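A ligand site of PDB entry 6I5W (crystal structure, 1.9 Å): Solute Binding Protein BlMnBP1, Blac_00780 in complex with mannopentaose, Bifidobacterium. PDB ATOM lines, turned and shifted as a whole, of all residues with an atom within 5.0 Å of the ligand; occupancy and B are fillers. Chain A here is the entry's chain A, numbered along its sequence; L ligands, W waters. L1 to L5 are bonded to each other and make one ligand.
Water W4 lies within hydrogen-bond range of O1 of LG4 L4, OE1 of Glu 117, O of Asp 304 and NZ of Lys 118. Water W1 lies within hydrogen-bond range of OH of Tyr 305 (2.8 Å) and O2 of LG2 L2 (2.8 Å). Water W5 lies within hydrogen-bond range of the side-chain amide oxygen of Gln 189 (2.8 Å) and an oxygen (O1) of LG3 L3 (2.9 Å). Water W2 bridges O of Asn 29 and O6 of LIG L1.
Merely in contact with the ligand: Ala 302, Asp 32, Arg 30, Trp 182, Thr 31, Gln 189, Lys 92 and Leu 376. Hydrophobic or aromatic side chains within 4 Å of the ligand: Trp 182, Trp 249, Trp 269, Ala 302, Tyr 305 and Leu 376. Within 4 Å of the ligand: Asn 29, Arg 30, Thr 31, Asp 32, Ser 65, Lys 92, Lys 118, Trp 182, Gln 189, Asn 203, Trp 249, Glu 250, Lys 253, Trp 269, Gln 273, Ala 302, Gly 303, Asp 304, Tyr 305, Asp 365, Leu 376 and Asn 388. The nearest printed residue that does not touch the ligand is Met 202 (4.1 Å).
The backbone carbonyl oxygen of Asp 304 sits close to an oxygen (O2) of LG3 L3. An oxygen (O5) of LG2 L2 is in hydrogen-bond range of the side-chain carboxylate (OD1) of Asp 304. The side-chain amide oxygen (OE1) of Gln 273 lies within hydrogen-bond range of an oxygen (O2) of LIG L1 (2.6 Å). NZ of Lys 118 sits at hydrogen-bond distance from O1 of LG4 L4 (2.8 Å). OE2 of Glu 250 lies within hydrogen-bond range of O1 of LIG L1, 2.9 Å away. ND2 of Asn 29 is in hydrogen-bond range of O4 of LG2 L2 (3.0 Å). OH of Tyr 305 lies within hydrogen-bond range of O5 of LG3 L3 (3.0 Å). An oxygen (O3) of LG5 L5 is in hydrogen-bond range of the side-chain amide oxygen of Asn 203 (3.0 Å). The backbone carbonyl oxygen of Gly 303 is in hydrogen-bond range of an oxygen (O2) of LG3 L3 (3.0 Å). O5 of LIG L1 sits at hydrogen-bond distance from NE1 of Trp 249. NZ of Lys 253 lies within hydrogen-bond range of O2 of LIG L1, at 3.0 Å. An oxygen (O5) of LG5 L5 is in hydrogen-bond range of the backbone carbonyl oxygen of Asn 388, at 3.1 Å. NE1 of Trp 269 lies within hydrogen-bond range of O1 of LG3 L3, at 3.3 Å. OD2 of Asp 365 is in hydrogen-bond range of O1 of LG5 L5, at 3.4 Å. OG of Ser 65 lies within hydrogen-bond range of O6 of LIG L1 (3.5 Å).
The side-chain amide oxygen (OE1) of Gln 273 sits at hydrogen-bond distance from the side-chain amino group (NZ) of Lys 253 (3.3 Å). The side-chain amide nitrogen (NE2) of Gln 273 sits close to the guanidinium group (NH1) of Arg 30 (3.2 Å). The side-chain carboxylate of Glu 250 is in salt-bridge range of the side-chain amino group of Lys 253 (3.7 Å). The backbone carbonyl oxygen (O) of Ala 302 sits at hydrogen-bond distance from the backbone NH (N) of Val 132 (2.9 Å). The side-chain carboxylate (OE2) of Glu 117 sits at hydrogen-bond distance from the backbone NH (N) of Gly 303. The side-chain amide nitrogen (ND2) of Asn 388 lies close to the backbone NH (N) of Gln 189, at 3.4 Å. OD2 of Asp 32 is in salt-bridge range of NH1 of Arg 30 (3.0 Å). The side-chain carboxylate (OE1) of Glu 180 is in hydrogen-bond range of the indole nitrogen (NE1) of Trp 182, at 2.6 Å.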
ATOM      1  N   ASN A  29     -12.875 -18.617   5.750  1.00  0.00           N
ATOM      2  CA  ASN A  29     -13.957 -19.228   6.488  1.00  0.00           C
ATOM      3  C   ASN A  29     -15.316 -18.600   6.219  1.00  0.00           C
ATOM      4  O   ASN A  29     -16.309 -19.048   6.781  1.00  0.00           O
ATOM      5  CB  ASN A  29     -13.708 -19.090   7.969  1.00  0.00           C
ATOM      6  CG  ASN A  29     -13.637 -17.655   8.380  1.00  0.00           C
ATOM      7  OD1 ASN A  29     -13.039 -16.857   7.718  1.00  0.00           O
ATOM      8  ND2 ASN A  29     -14.308 -17.312   9.504  1.00  0.00           N
ATOM      9  N   ARG A  30     -15.379 -17.543   5.424  1.00  0.00           N
ATOM     10  CA  ARG A  30     -16.658 -16.842   5.247  1.00  0.00           C
ATOM     11  C   ARG A  30     -17.414 -17.435   4.066  1.00  0.00           C
ATOM     12  O   ARG A  30     -17.681 -16.803   3.048  1.00  0.00           O
ATOM     13  CB  ARG A  30     -16.430 -15.340   5.081  1.00  0.00           C
ATOM     14  CG  ARG A  30     -15.777 -14.619   6.265  1.00  0.00           C
ATOM     15  CD  ARG A  30     -16.678 -14.687   7.528  1.00  0.00           C
ATOM     16  NE  ARG A  30     -17.996 -14.155   7.223  1.00  0.00           N
ATOM     17  CZ  ARG A  30     -18.335 -12.874   7.317  1.00  0.00           C
ATOM     18  NH1 ARG A  30     -19.571 -12.478   7.033  1.00  0.00           N
ATOM     19  NH2 ARG A  30     -17.420 -11.998   7.740  1.00  0.00           N
ATOM     20  N   THR A  31     -17.798 -18.709   4.219  1.00  0.00           N
ATOM     21  CA  THR A  31     -18.701 -19.338   3.267  1.00  0.00           C
ATOM     22  C   THR A  31     -19.893 -18.441   2.933  1.00  0.00           C
ATOM     23  O   THR A  31     -20.287 -18.352   1.771  1.00  0.00           O
ATOM     24  CB  THR A  31     -19.181 -20.694   3.826  1.00  0.00           C
ATOM     25  OG1 THR A  31     -19.899 -20.503   5.052  1.00  0.00           O
ATOM     26  CG2 THR A  31     -17.974 -21.645   4.039  1.00  0.00           C
ATOM     27  N   ASP A  32     -20.489 -17.755   3.948  1.00  0.00           N
ATOM     28  CA  ASP A  32     -21.638 -16.903   3.647  1.00  0.00           C
ATOM     29  C   ASP A  32     -21.303 -15.836   2.617  1.00  0.00           C
ATOM     30  O   ASP A  32     -22.150 -15.459   1.801  1.00  0.00           O
ATOM     31  CB  ASP A  32     -22.187 -16.249   4.911  1.00  0.00           C
ATOM     32  CG  ASP A  32     -21.154 -15.450   5.694  1.00  0.00           C
ATOM     33  OD1 ASP A  32     -19.954 -15.693   5.509  1.00  0.00           O
ATOM     34  OD2 ASP A  32     -21.576 -14.606   6.554  1.00  0.00           O
ATOM     35  N   SER A  65     -16.748 -24.877   5.159  1.00  0.00           N
ATOM     36  CA  SER A  65     -17.259 -25.000   6.516  1.00  0.00           C
ATOM     37  C   SER A  65     -16.387 -25.961   7.300  1.00  0.00           C
ATOM     38  O   SER A  65     -15.767 -26.867   6.745  1.00  0.00           O
ATOM     39  CB  SER A  65     -18.707 -25.468   6.518  1.00  0.00           C
ATOM     40  OG  SER A  65     -19.573 -24.349   6.425  1.00  0.00           O
ATOM     41  N   ASN A  66     -16.329 -25.773   8.592  1.00  0.00           N
ATOM     42  CA  ASN A  66     -15.281 -26.417   9.373  1.00  0.00           C
ATOM     43  C   ASN A  66     -13.945 -25.957   8.795  1.00  0.00           C
ATOM     44  O   ASN A  66     -13.098 -26.764   8.385  1.00  0.00           O
ATOM     45  CB  ASN A  66     -15.401 -27.929   9.366  1.00  0.00           C
ATOM     46  CG  ASN A  66     -14.435 -28.567  10.344  1.00  0.00           C
ATOM     47  OD1 ASN A  66     -14.021 -27.941  11.331  1.00  0.00           O
ATOM     48  ND2 ASN A  66     -14.074 -29.818  10.075  1.00  0.00           N
ATOM     49  N   LYS A  92       2.848 -20.297  17.144  1.00  0.00           N
ATOM     50  CA  LYS A  92       3.509 -19.129  16.584  1.00  0.00           C
ATOM     51  C   LYS A  92       4.890 -19.483  16.019  1.00  0.00           C
ATOM     52  O   LYS A  92       5.416 -18.764  15.166  1.00  0.00           O
ATOM     53  CB  LYS A  92       3.642 -18.036  17.650  1.00  0.00           C
ATOM     54  CG  LYS A  92       2.428 -17.850  18.639  1.00  0.00           C
ATOM     55  CD  LYS A  92       1.137 -17.318  17.969  1.00  0.00           C
ATOM     56  CE  LYS A  92      -0.141 -17.697  18.752  1.00  0.00           C
ATOM     57  NZ  LYS A  92      -1.363 -17.750  17.875  1.00  0.00           N
ATOM     58  N   GLU A 117       0.500  -9.847  16.881  1.00  0.00           N
ATOM     59  CA  GLU A 117      -0.402 -10.960  17.167  1.00  0.00           C
ATOM     60  C   GLU A 117       0.064 -12.218  16.439  1.00  0.00           C
ATOM     61  O   GLU A 117       0.294 -13.270  17.042  1.00  0.00           O
ATOM     62  CB  GLU A 117      -1.826 -10.576  16.778  1.00  0.00           C
ATOM     63  CG  GLU A 117      -2.877 -11.487  17.358  1.00  0.00           C
ATOM     64  CD  GLU A 117      -4.294 -11.115  16.951  1.00  0.00           C
ATOM     65  OE1 GLU A 117      -4.652 -11.334  15.770  1.00  0.00           O
ATOM     66  OE2 GLU A 117      -5.044 -10.623  17.826  1.00  0.00           O
ATOM     67  N   LYS A 118       0.210 -12.131  15.126  1.00  0.00           N
ATOM     68  CA  LYS A 118       0.685 -13.260  14.323  1.00  0.00           C
ATOM     69  C   LYS A 118       2.133 -13.004  13.942  1.00  0.00           C
ATOM     70  O   LYS A 118       2.489 -12.770  12.788  1.00  0.00           O
ATOM     71  CB  LYS A 118      -0.180 -13.476  13.095  1.00  0.00           C
ATOM     72  CG  LYS A 118      -1.650 -13.702  13.410  1.00  0.00           C
ATOM     73  CD  LYS A 118      -1.853 -15.016  14.130  1.00  0.00           C
ATOM     74  CE  LYS A 118      -3.301 -15.483  14.065  1.00  0.00           C
ATOM     75  NZ  LYS A 118      -3.834 -15.707  15.452  1.00  0.00           N
ATOM     76  N   VAL A 132     -11.669  -7.166  16.580  1.00  0.00           N
ATOM     77  CA  VAL A 132     -12.928  -7.515  17.225  1.00  0.00           C
ATOM     78  C   VAL A 132     -12.781  -7.632  18.744  1.00  0.00           C
ATOM     79  O   VAL A 132     -11.716  -7.964  19.281  1.00  0.00           O
ATOM     80  CB  VAL A 132     -13.515  -8.825  16.650  1.00  0.00           C
ATOM     81  CG1 VAL A 132     -13.898  -8.622  15.190  1.00  0.00           C
ATOM     82  CG2 VAL A 132     -12.510  -9.930  16.806  1.00  0.00           C
ATOM     83  N   GLU A 180     -21.634 -26.250  16.566  1.00  0.00           N
ATOM     84  CA  GLU A 180     -20.504 -25.603  15.942  1.00  0.00           C
ATOM     85  C   GLU A 180     -19.340 -25.619  16.933  1.00  0.00           C
ATOM     86  O   GLU A 180     -19.350 -24.865  17.900  1.00  0.00           O
ATOM     87  CB  GLU A 180     -20.848 -24.178  15.530  1.00  0.00           C
ATOM     88  CG  GLU A 180     -21.939 -24.088  14.452  1.00  0.00           C
ATOM     89  CD  GLU A 180     -21.507 -24.692  13.088  1.00  0.00           C
ATOM     90  OE1 GLU A 180     -20.392 -24.384  12.610  1.00  0.00           O
ATOM     91  OE2 GLU A 180     -22.290 -25.470  12.502  1.00  0.00           O
ATOM     92  N   TRP A 182     -16.492 -24.406  16.635  1.00  0.00           N
ATOM     93  CA  TRP A 182     -15.886 -23.076  16.807  1.00  0.00           C
ATOM     94  C   TRP A 182     -16.721 -22.160  17.697  1.00  0.00           C
ATOM     95  O   TRP A 182     -16.159 -21.259  18.319  1.00  0.00           O
ATOM     96  CB  TRP A 182     -15.659 -22.438  15.448  1.00  0.00           C
ATOM     97  CG  TRP A 182     -16.879 -22.316  14.653  1.00  0.00           C
ATOM     98  CD1 TRP A 182     -17.300 -23.145  13.694  1.00  0.00           C
ATOM     99  CD2 TRP A 182     -17.876 -21.292  14.777  1.00  0.00           C
ATOM    100  NE1 TRP A 182     -18.498 -22.723  13.182  1.00  0.00           N
ATOM    101  CE2 TRP A 182     -18.877 -21.571  13.822  1.00  0.00           C
ATOM    102  CE3 TRP A 182     -18.007 -20.150  15.564  1.00  0.00           C
ATOM    103  CZ2 TRP A 182     -19.972 -20.751  13.628  1.00  0.00           C
ATOM    104  CZ3 TRP A 182     -19.159 -19.356  15.408  1.00  0.00           C
ATOM    105  CH2 TRP A 182     -20.106 -19.655  14.436  1.00  0.00           C
ATOM    106  N   GLN A 189     -11.993 -17.328  24.655  1.00  0.00           N
ATOM    107  CA  GLN A 189     -11.524 -15.973  24.342  1.00  0.00           C
ATOM    108  C   GLN A 189     -11.896 -14.962  25.407  1.00  0.00           C
ATOM    109  O   GLN A 189     -11.440 -13.821  25.320  1.00  0.00           O
ATOM    110  CB  GLN A 189     -12.126 -15.537  23.001  1.00  0.00           C
ATOM    111  CG  GLN A 189     -11.651 -16.413  21.804  1.00  0.00           C
ATOM    112  CD  GLN A 189     -12.493 -16.239  20.546  1.00  0.00           C
ATOM    113  OE1 GLN A 189     -13.309 -15.306  20.432  1.00  0.00           O
ATOM    114  NE2 GLN A 189     -12.295 -17.150  19.588  1.00  0.00           N
ATOM    115  N   MET A 202      -3.105 -13.811  29.413  1.00  0.00           N
ATOM    116  CA  MET A 202      -3.158 -14.891  28.427  1.00  0.00           C
ATOM    117  C   MET A 202      -1.774 -15.489  28.162  1.00  0.00           C
ATOM    118  O   MET A 202      -1.618 -16.707  28.056  1.00  0.00           O
ATOM    119  CB  MET A 202      -3.749 -14.356  27.112  1.00  0.00           C
ATOM    120  CG  MET A 202      -4.100 -15.385  26.032  1.00  0.00           C
ATOM    121  SD  MET A 202      -5.257 -16.648  26.603  1.00  0.00           S
ATOM    122  CE  MET A 202      -6.689 -16.371  25.563  1.00  0.00           C
ATOM    123  N   ASN A 203      -0.743 -14.651  28.050  1.00  0.00           N
ATOM    124  CA  ASN A 203       0.533 -15.119  27.541  1.00  0.00           C
ATOM    125  C   ASN A 203       1.620 -15.258  28.588  1.00  0.00           C
ATOM    126  O   ASN A 203       2.614 -15.943  28.316  1.00  0.00           O
ATOM    127  CB  ASN A 203       1.039 -14.190  26.435  1.00  0.00           C
ATOM    128  CG  ASN A 203       0.219 -14.325  25.186  1.00  0.00           C
ATOM    129  OD1 ASN A 203      -0.210 -15.438  24.835  1.00  0.00           O
ATOM    130  ND2 ASN A 203      -0.040 -13.213  24.519  1.00  0.00           N
ATOM    131  N   TRP A 249     -26.330 -23.108  13.277  1.00  0.00           N
ATOM    132  CA  TRP A 249     -25.766 -21.767  13.275  1.00  0.00           C
ATOM    133  C   TRP A 249     -26.484 -20.833  12.309  1.00  0.00           C
ATOM    134  O   TRP A 249     -26.851 -19.713  12.684  1.00  0.00           O
ATOM    135  CB  TRP A 249     -24.286 -21.879  12.967  1.00  0.00           C
ATOM    136  CG  TRP A 249     -23.618 -20.673  12.525  1.00  0.00           C
ATOM    137  CD1 TRP A 249     -22.991 -20.512  11.313  1.00  0.00           C
ATOM    138  CD2 TRP A 249     -23.439 -19.457  13.240  1.00  0.00           C
ATOM    139  NE1 TRP A 249     -22.441 -19.264  11.241  1.00  0.00           N
ATOM    140  CE2 TRP A 249     -22.714 -18.591  12.403  1.00  0.00           C
ATOM    141  CE3 TRP A 249     -23.847 -18.997  14.496  1.00  0.00           C
ATOM    142  CZ2 TRP A 249     -22.384 -17.292  12.801  1.00  0.00           C
ATOM    143  CZ3 TRP A 249     -23.521 -17.688  14.874  1.00  0.00           C
ATOM    144  CH2 TRP A 249     -22.778 -16.868  14.024  1.00  0.00           C
ATOM    145  N   GLU A 250     -26.654 -21.241  11.052  1.00  0.00           N
ATOM    146  CA  GLU A 250     -27.216 -20.297  10.097  1.00  0.00           C
ATOM    147  C   GLU A 250     -28.613 -19.866  10.536  1.00  0.00           C
ATOM    148  O   GLU A 250     -28.964 -18.683  10.536  1.00  0.00           O
ATOM    149  CB  GLU A 250     -27.244 -20.883   8.695  1.00  0.00           C
ATOM    150  CG  GLU A 250     -25.994 -20.575   7.877  1.00  0.00           C
ATOM    151  CD  GLU A 250     -25.837 -19.088   7.587  1.00  0.00           C
ATOM    152  OE1 GLU A 250     -26.850 -18.437   7.209  1.00  0.00           O
ATOM    153  OE2 GLU A 250     -24.711 -18.570   7.766  1.00  0.00           O
ATOM    154  N   LYS A 253     -28.909 -17.222  13.377  1.00  0.00           N
ATOM    155  CA  LYS A 253     -28.848 -15.804  13.046  1.00  0.00           C
ATOM    156  C   LYS A 253     -30.247 -15.262  12.804  1.00  0.00           C
ATOM    157  O   LYS A 253     -30.617 -14.200  13.323  1.00  0.00           O
ATOM    158  CB  LYS A 253     -27.969 -15.571  11.807  1.00  0.00           C
ATOM    159  CG  LYS A 253     -26.663 -16.406  11.717  1.00  0.00           C
ATOM    160  CD  LYS A 253     -26.056 -16.213  10.333  1.00  0.00           C
ATOM    161  CE  LYS A 253     -24.610 -16.553  10.289  1.00  0.00           C
ATOM    162  NZ  LYS A 253     -24.085 -16.559   8.868  1.00  0.00           N
ATOM    163  N   TRP A 269     -17.707  -9.597  15.476  1.00  0.00           N
ATOM    164  CA  TRP A 269     -17.961  -9.908  14.072  1.00  0.00           C
ATOM    165  C   TRP A 269     -19.374 -10.444  13.852  1.00  0.00           C
ATOM    166  O   TRP A 269     -19.889 -10.400  12.731  1.00  0.00           O
ATOM    167  CB  TRP A 269     -16.962 -10.968  13.583  1.00  0.00           C
ATOM    168  CG  TRP A 269     -16.985 -12.238  14.380  1.00  0.00           C
ATOM    169  CD1 TRP A 269     -16.189 -12.544  15.469  1.00  0.00           C
ATOM    170  CD2 TRP A 269     -17.857 -13.327  14.204  1.00  0.00           C
ATOM    171  NE1 TRP A 269     -16.531 -13.772  15.942  1.00  0.00           N
ATOM    172  CE2 TRP A 269     -17.559 -14.270  15.188  1.00  0.00           C
ATOM    173  CE3 TRP A 269     -18.885 -13.595  13.303  1.00  0.00           C
ATOM    174  CZ2 TRP A 269     -18.222 -15.463  15.297  1.00  0.00           C
ATOM    175  CZ3 TRP A 269     -19.553 -14.795  13.409  1.00  0.00           C
ATOM    176  CH2 TRP A 269     -19.239 -15.705  14.412  1.00  0.00           C
ATOM    177  N   GLN A 273     -23.849  -9.928  11.080  1.00  0.00           N
ATOM    178  CA  GLN A 273     -24.480 -11.103  10.516  1.00  0.00           C
ATOM    179  C   GLN A 273     -25.850 -11.345  11.135  1.00  0.00           C
ATOM    180  O   GLN A 273     -26.786 -11.788  10.460  1.00  0.00           O
ATOM    181  CB  GLN A 273     -23.585 -12.336  10.701  1.00  0.00           C
ATOM    182  CG  GLN A 273     -22.107 -12.087  10.507  1.00  0.00           C
ATOM    183  CD  GLN A 273     -21.336 -13.363  10.260  1.00  0.00           C
ATOM    184  OE1 GLN A 273     -21.903 -14.465  10.229  1.00  0.00           O
ATOM    185  NE2 GLN A 273     -20.035 -13.231  10.062  1.00  0.00           N
ATOM    186  N   ALA A 302      -8.826  -8.250  19.768  1.00  0.00           N
ATOM    187  CA  ALA A 302      -7.953  -9.227  19.085  1.00  0.00           C
ATOM    188  C   ALA A 302      -8.371  -9.313  17.622  1.00  0.00           C
ATOM    189  O   ALA A 302      -9.443  -8.841  17.274  1.00  0.00           O
ATOM    190  CB  ALA A 302      -8.022 -10.557  19.790  1.00  0.00           C
ATOM    191  N   GLY A 303      -7.551  -9.913  16.792  1.00  0.00           N
ATOM    192  CA  GLY A 303      -7.882 -10.057  15.377  1.00  0.00           C
ATOM    193  C   GLY A 303      -8.961 -11.091  15.185  1.00  0.00           C
ATOM    194  O   GLY A 303      -9.094 -11.976  16.012  1.00  0.00           O
ATOM    195  N   ASP A 304      -9.718 -10.963  14.076  1.00  0.00           N
ATOM    196  CA  ASP A 304     -10.766 -11.913  13.624  1.00  0.00           C
ATOM    197  C   ASP A 304     -10.010 -13.105  13.037  1.00  0.00           C
ATOM    198  O   ASP A 304      -9.560 -13.953  13.834  1.00  0.00           O
ATOM    199  CB  ASP A 304     -11.731 -11.270  12.632  1.00  0.00           C
ATOM    200  CG  ASP A 304     -12.893 -12.160  12.242  1.00  0.00           C
ATOM    201  OD1 ASP A 304     -12.677 -13.374  12.053  1.00  0.00           O
ATOM    202  OD2 ASP A 304     -14.026 -11.637  12.138  1.00  0.00           O
ATOM    203  N   TYR A 305      -9.854 -13.187  11.704  1.00  0.00           N
ATOM    204  CA  TYR A 305      -8.985 -14.183  11.075  1.00  0.00           C
ATOM    205  C   TYR A 305      -7.883 -13.346  10.422  1.00  0.00           C
ATOM    206  O   TYR A 305      -8.143 -12.265   9.962  1.00  0.00           O
ATOM    207  CB  TYR A 305      -9.787 -15.079  10.139  1.00  0.00           C
ATOM    208  CG  TYR A 305     -10.056 -16.454  10.682  1.00  0.00           C
ATOM    209  CD1 TYR A 305      -9.032 -17.352  10.873  1.00  0.00           C
ATOM    210  CD2 TYR A 305     -11.338 -16.879  10.977  1.00  0.00           C
ATOM    211  CE1 TYR A 305      -9.266 -18.625  11.356  1.00  0.00           C
ATOM    212  CE2 TYR A 305     -11.593 -18.141  11.440  1.00  0.00           C
ATOM    213  CZ  TYR A 305     -10.557 -19.023  11.637  1.00  0.00           C
ATOM    214  OH  TYR A 305     -10.782 -20.279  12.096  1.00  0.00           O
ATOM    215  N   ASP A 365      -4.033  -8.309  24.623  1.00  0.00           N
ATOM    216  CA  ASP A 365      -3.087  -9.219  25.245  1.00  0.00           C
ATOM    217  C   ASP A 365      -1.644  -8.814  24.958  1.00  0.00           C
ATOM    218  O   ASP A 365      -1.248  -8.596  23.803  1.00  0.00           O
ATOM    219  CB  ASP A 365      -3.354 -10.647  24.757  1.00  0.00           C
ATOM    220  CG  ASP A 365      -4.660 -11.190  25.288  1.00  0.00           C
ATOM    221  OD1 ASP A 365      -5.082 -10.657  26.328  1.00  0.00           O
ATOM    222  OD2 ASP A 365      -5.255 -12.119  24.698  1.00  0.00           O
ATOM    223  N   LEU A 376       2.926 -20.716  26.277  1.00  0.00           N
ATOM    224  CA  LEU A 376       1.505 -21.006  26.275  1.00  0.00           C
ATOM    225  C   LEU A 376       1.161 -22.157  25.349  1.00  0.00           C
ATOM    226  O   LEU A 376       0.323 -23.000  25.695  1.00  0.00           O
ATOM    227  CB  LEU A 376       0.729 -19.776  25.845  1.00  0.00           C
ATOM    228  CG  LEU A 376      -0.767 -20.038  25.718  1.00  0.00           C
ATOM    229  CD1 LEU A 376      -1.362 -20.688  26.977  1.00  0.00           C
ATOM    230  CD2 LEU A 376      -1.457 -18.718  25.395  1.00  0.00           C
ATOM    231  N   ASN A 380      -0.402 -25.670  26.602  1.00  0.00           N
ATOM    232  CA  ASN A 380      -1.610 -26.084  25.873  1.00  0.00           C
ATOM    233  C   ASN A 380      -1.494 -27.482  25.320  1.00  0.00           C
ATOM    234  O   ASN A 380      -2.433 -28.287  25.437  1.00  0.00           O
ATOM    235  CB  ASN A 380      -1.858 -25.120  24.714  1.00  0.00           C
ATOM    236  CG  ASN A 380      -3.201 -24.475  24.790  1.00  0.00           C
ATOM    237  OD1 ASN A 380      -4.075 -24.850  25.598  1.00  0.00           O
ATOM    238  ND2 ASN A 380      -3.400 -23.479  23.946  1.00  0.00           N
ATOM    239  N   ILE A 387      -6.617 -24.456  25.076  1.00  0.00           N
ATOM    240  CA  ILE A 387      -7.179 -23.130  25.465  1.00  0.00           C
ATOM    241  C   ILE A 387      -7.073 -22.207  24.243  1.00  0.00           C
ATOM    242  O   ILE A 387      -5.995 -22.097  23.739  1.00  0.00           O
ATOM    243  CB  ILE A 387      -6.450 -22.558  26.681  1.00  0.00           C
ATOM    244  CG1 ILE A 387      -6.683 -23.407  27.922  1.00  0.00           C
ATOM    245  CG2 ILE A 387      -6.844 -21.120  26.906  1.00  0.00           C
ATOM    246  CD1 ILE A 387      -8.126 -23.492  28.295  1.00  0.00           C
ATOM    247  N   ASN A 388      -8.168 -21.597  23.791  1.00  0.00           N
ATOM    248  CA  ASN A 388      -8.186 -20.668  22.650  1.00  0.00           C
ATOM    249  C   ASN A 388      -7.493 -21.319  21.468  1.00  0.00           C
ATOM    250  O   ASN A 388      -6.611 -20.703  20.892  1.00  0.00           O
ATOM    251  CB  ASN A 388      -7.484 -19.355  22.975  1.00  0.00           C
ATOM    252  CG  ASN A 388      -8.377 -18.186  22.686  1.00  0.00           C
ATOM    253  OD1 ASN A 388      -8.765 -17.992  21.545  1.00  0.00           O
ATOM    254  ND2 ASN A 388      -8.710 -17.432  23.697  1.00  0.00           N
HETATM  255  C1  LIG L   1     -20.620 -18.411   7.897  1.00  0.00           C
HETATM  256  C2  LIG L   1     -20.244 -17.136   8.620  1.00  0.00           C
HETATM  257  C3  LIG L   1     -18.863 -17.335   9.277  1.00  0.00           C
HETATM  258  C4  LIG L   1     -18.814 -18.620  10.045  1.00  0.00           C
HETATM  259  C5  LIG L   1     -19.304 -19.809   9.190  1.00  0.00           C
HETATM  260  C6  LIG L   1     -19.298 -21.073   9.984  1.00  0.00           C
HETATM  261  O1  LIG L   1     -21.900 -18.152   7.420  1.00  0.00           O
HETATM  262  O2  LIG L   1     -21.163 -16.929   9.629  1.00  0.00           O
HETATM  263  O3  LIG L   1     -18.619 -16.181  10.089  1.00  0.00           O
HETATM  264  O4  LIG L   1     -17.536 -18.920  10.463  1.00  0.00           O
HETATM  265  O5  LIG L   1     -20.645 -19.473   8.831  1.00  0.00           O
HETATM  266  O6  LIG L   1     -19.316 -22.180   9.127  1.00  0.00           O
HETATM  267  C1  LG2 L   2     -17.139 -18.249  11.786  1.00  0.00           C
HETATM  268  C2  LG2 L   2     -16.140 -19.166  12.456  1.00  0.00           C
HETATM  269  C3  LG2 L   2     -15.475 -18.429  13.579  1.00  0.00           C
HETATM  270  C4  LG2 L   2     -14.962 -17.066  13.168  1.00  0.00           C
HETATM  271  C5  LG2 L   2     -16.079 -16.305  12.487  1.00  0.00           C
HETATM  272  C6  LG2 L   2     -15.699 -14.908  12.008  1.00  0.00           C
HETATM  273  O1  LG2 L   2     -15.155 -19.518  11.456  1.00  0.00           O
HETATM  274  O2  LG2 L   2     -14.483 -19.225  14.094  1.00  0.00           O
HETATM  275  O3  LG2 L   2     -14.597 -16.346  14.332  1.00  0.00           O
HETATM  276  O4  LG2 L   2     -16.568 -17.094  11.393  1.00  0.00           O
HETATM  277  O5  LG2 L   2     -14.457 -14.939  11.262  1.00  0.00           O
HETATM  278  C1  LG3 L   3     -13.110 -16.284  14.578  1.00  0.00           C
HETATM  279  C2  LG3 L   3     -12.977 -15.095  15.474  1.00  0.00           C
HETATM  280  C3  LG3 L   3     -11.494 -14.953  15.724  1.00  0.00           C
HETATM  281  C4  LG3 L   3     -10.804 -16.236  16.120  1.00  0.00           C
HETATM  282  C5  LG3 L   3     -11.212 -17.430  15.256  1.00  0.00           C
HETATM  283  C6  LG3 L   3     -10.784 -18.734  15.859  1.00  0.00           C
HETATM  284  O1  LG3 L   3     -13.659 -15.222  16.738  1.00  0.00           O
HETATM  285  O2  LG3 L   3     -11.245 -13.939  16.707  1.00  0.00           O
HETATM  286  O3  LG3 L   3      -9.400 -16.001  15.839  1.00  0.00           O
HETATM  287  O4  LG3 L   3     -12.607 -17.414  15.165  1.00  0.00           O
HETATM  288  O5  LG3 L   3     -11.124 -19.751  14.987  1.00  0.00           O
HETATM  289  C1  LG4 L   4      -8.717 -16.457  16.920  1.00  0.00           C
HETATM  290  C2  LG4 L   4      -7.193 -16.740  16.595  1.00  0.00           C
HETATM  291  C3  LG4 L   4      -6.426 -16.838  17.932  1.00  0.00           C
HETATM  292  C4  LG4 L   4      -6.786 -15.551  18.784  1.00  0.00           C
HETATM  293  C5  LG4 L   4      -8.295 -15.659  19.105  1.00  0.00           C
HETATM  294  C6  LG4 L   4      -8.774 -14.737  20.167  1.00  0.00           C
HETATM  295  O1  LG4 L   4      -6.626 -15.652  15.826  1.00  0.00           O
HETATM  296  O2  LG4 L   4      -5.053 -17.057  17.757  1.00  0.00           O
HETATM  297  O3  LG4 L   4      -6.057 -15.407  19.952  1.00  0.00           O
HETATM  298  O4  LG4 L   4      -8.916 -15.395  17.868  1.00  0.00           O
HETATM  299  O5  LG4 L   4      -8.318 -13.453  19.859  1.00  0.00           O
HETATM  300  C1  LG5 L   5      -4.843 -15.236  20.366  1.00  0.00           C
HETATM  301  C2  LG5 L   5      -3.932 -14.086  20.709  1.00  0.00           C
HETATM  302  C3  LG5 L   5      -2.653 -14.578  21.399  1.00  0.00           C
HETATM  303  C4  LG5 L   5      -2.781 -15.863  22.203  1.00  0.00           C
HETATM  304  C5  LG5 L   5      -3.707 -16.868  21.534  1.00  0.00           C
HETATM  305  C6  LG5 L   5      -3.954 -18.097  22.383  1.00  0.00           C
HETATM  306  O1  LG5 L   5      -4.553 -13.152  21.551  1.00  0.00           O
HETATM  307  O2  LG5 L   5      -2.139 -13.559  22.274  1.00  0.00           O
HETATM  308  O3  LG5 L   5      -1.484 -16.443  22.340  1.00  0.00           O
HETATM  309  O4  LG5 L   5      -4.916 -16.178  21.352  1.00  0.00           O
HETATM  310  O5  LG5 L   5      -3.984 -19.233  21.522  1.00  0.00           O
HETATM  311  O   HOH W   1     -13.196 -21.403  12.893  1.00  0.00           O
HETATM  312  O   HOH W   2     -16.466 -21.462   7.822  1.00  0.00           O
HETATM  313  O   HOH W   3     -12.163 -22.541  15.410  1.00  0.00           O
HETATM  314  O   HOH W   4      -6.320 -13.572  14.334  1.00  0.00           O
HETATM  315  O   HOH W   5     -14.166 -13.224  18.784  1.00  0.00           O
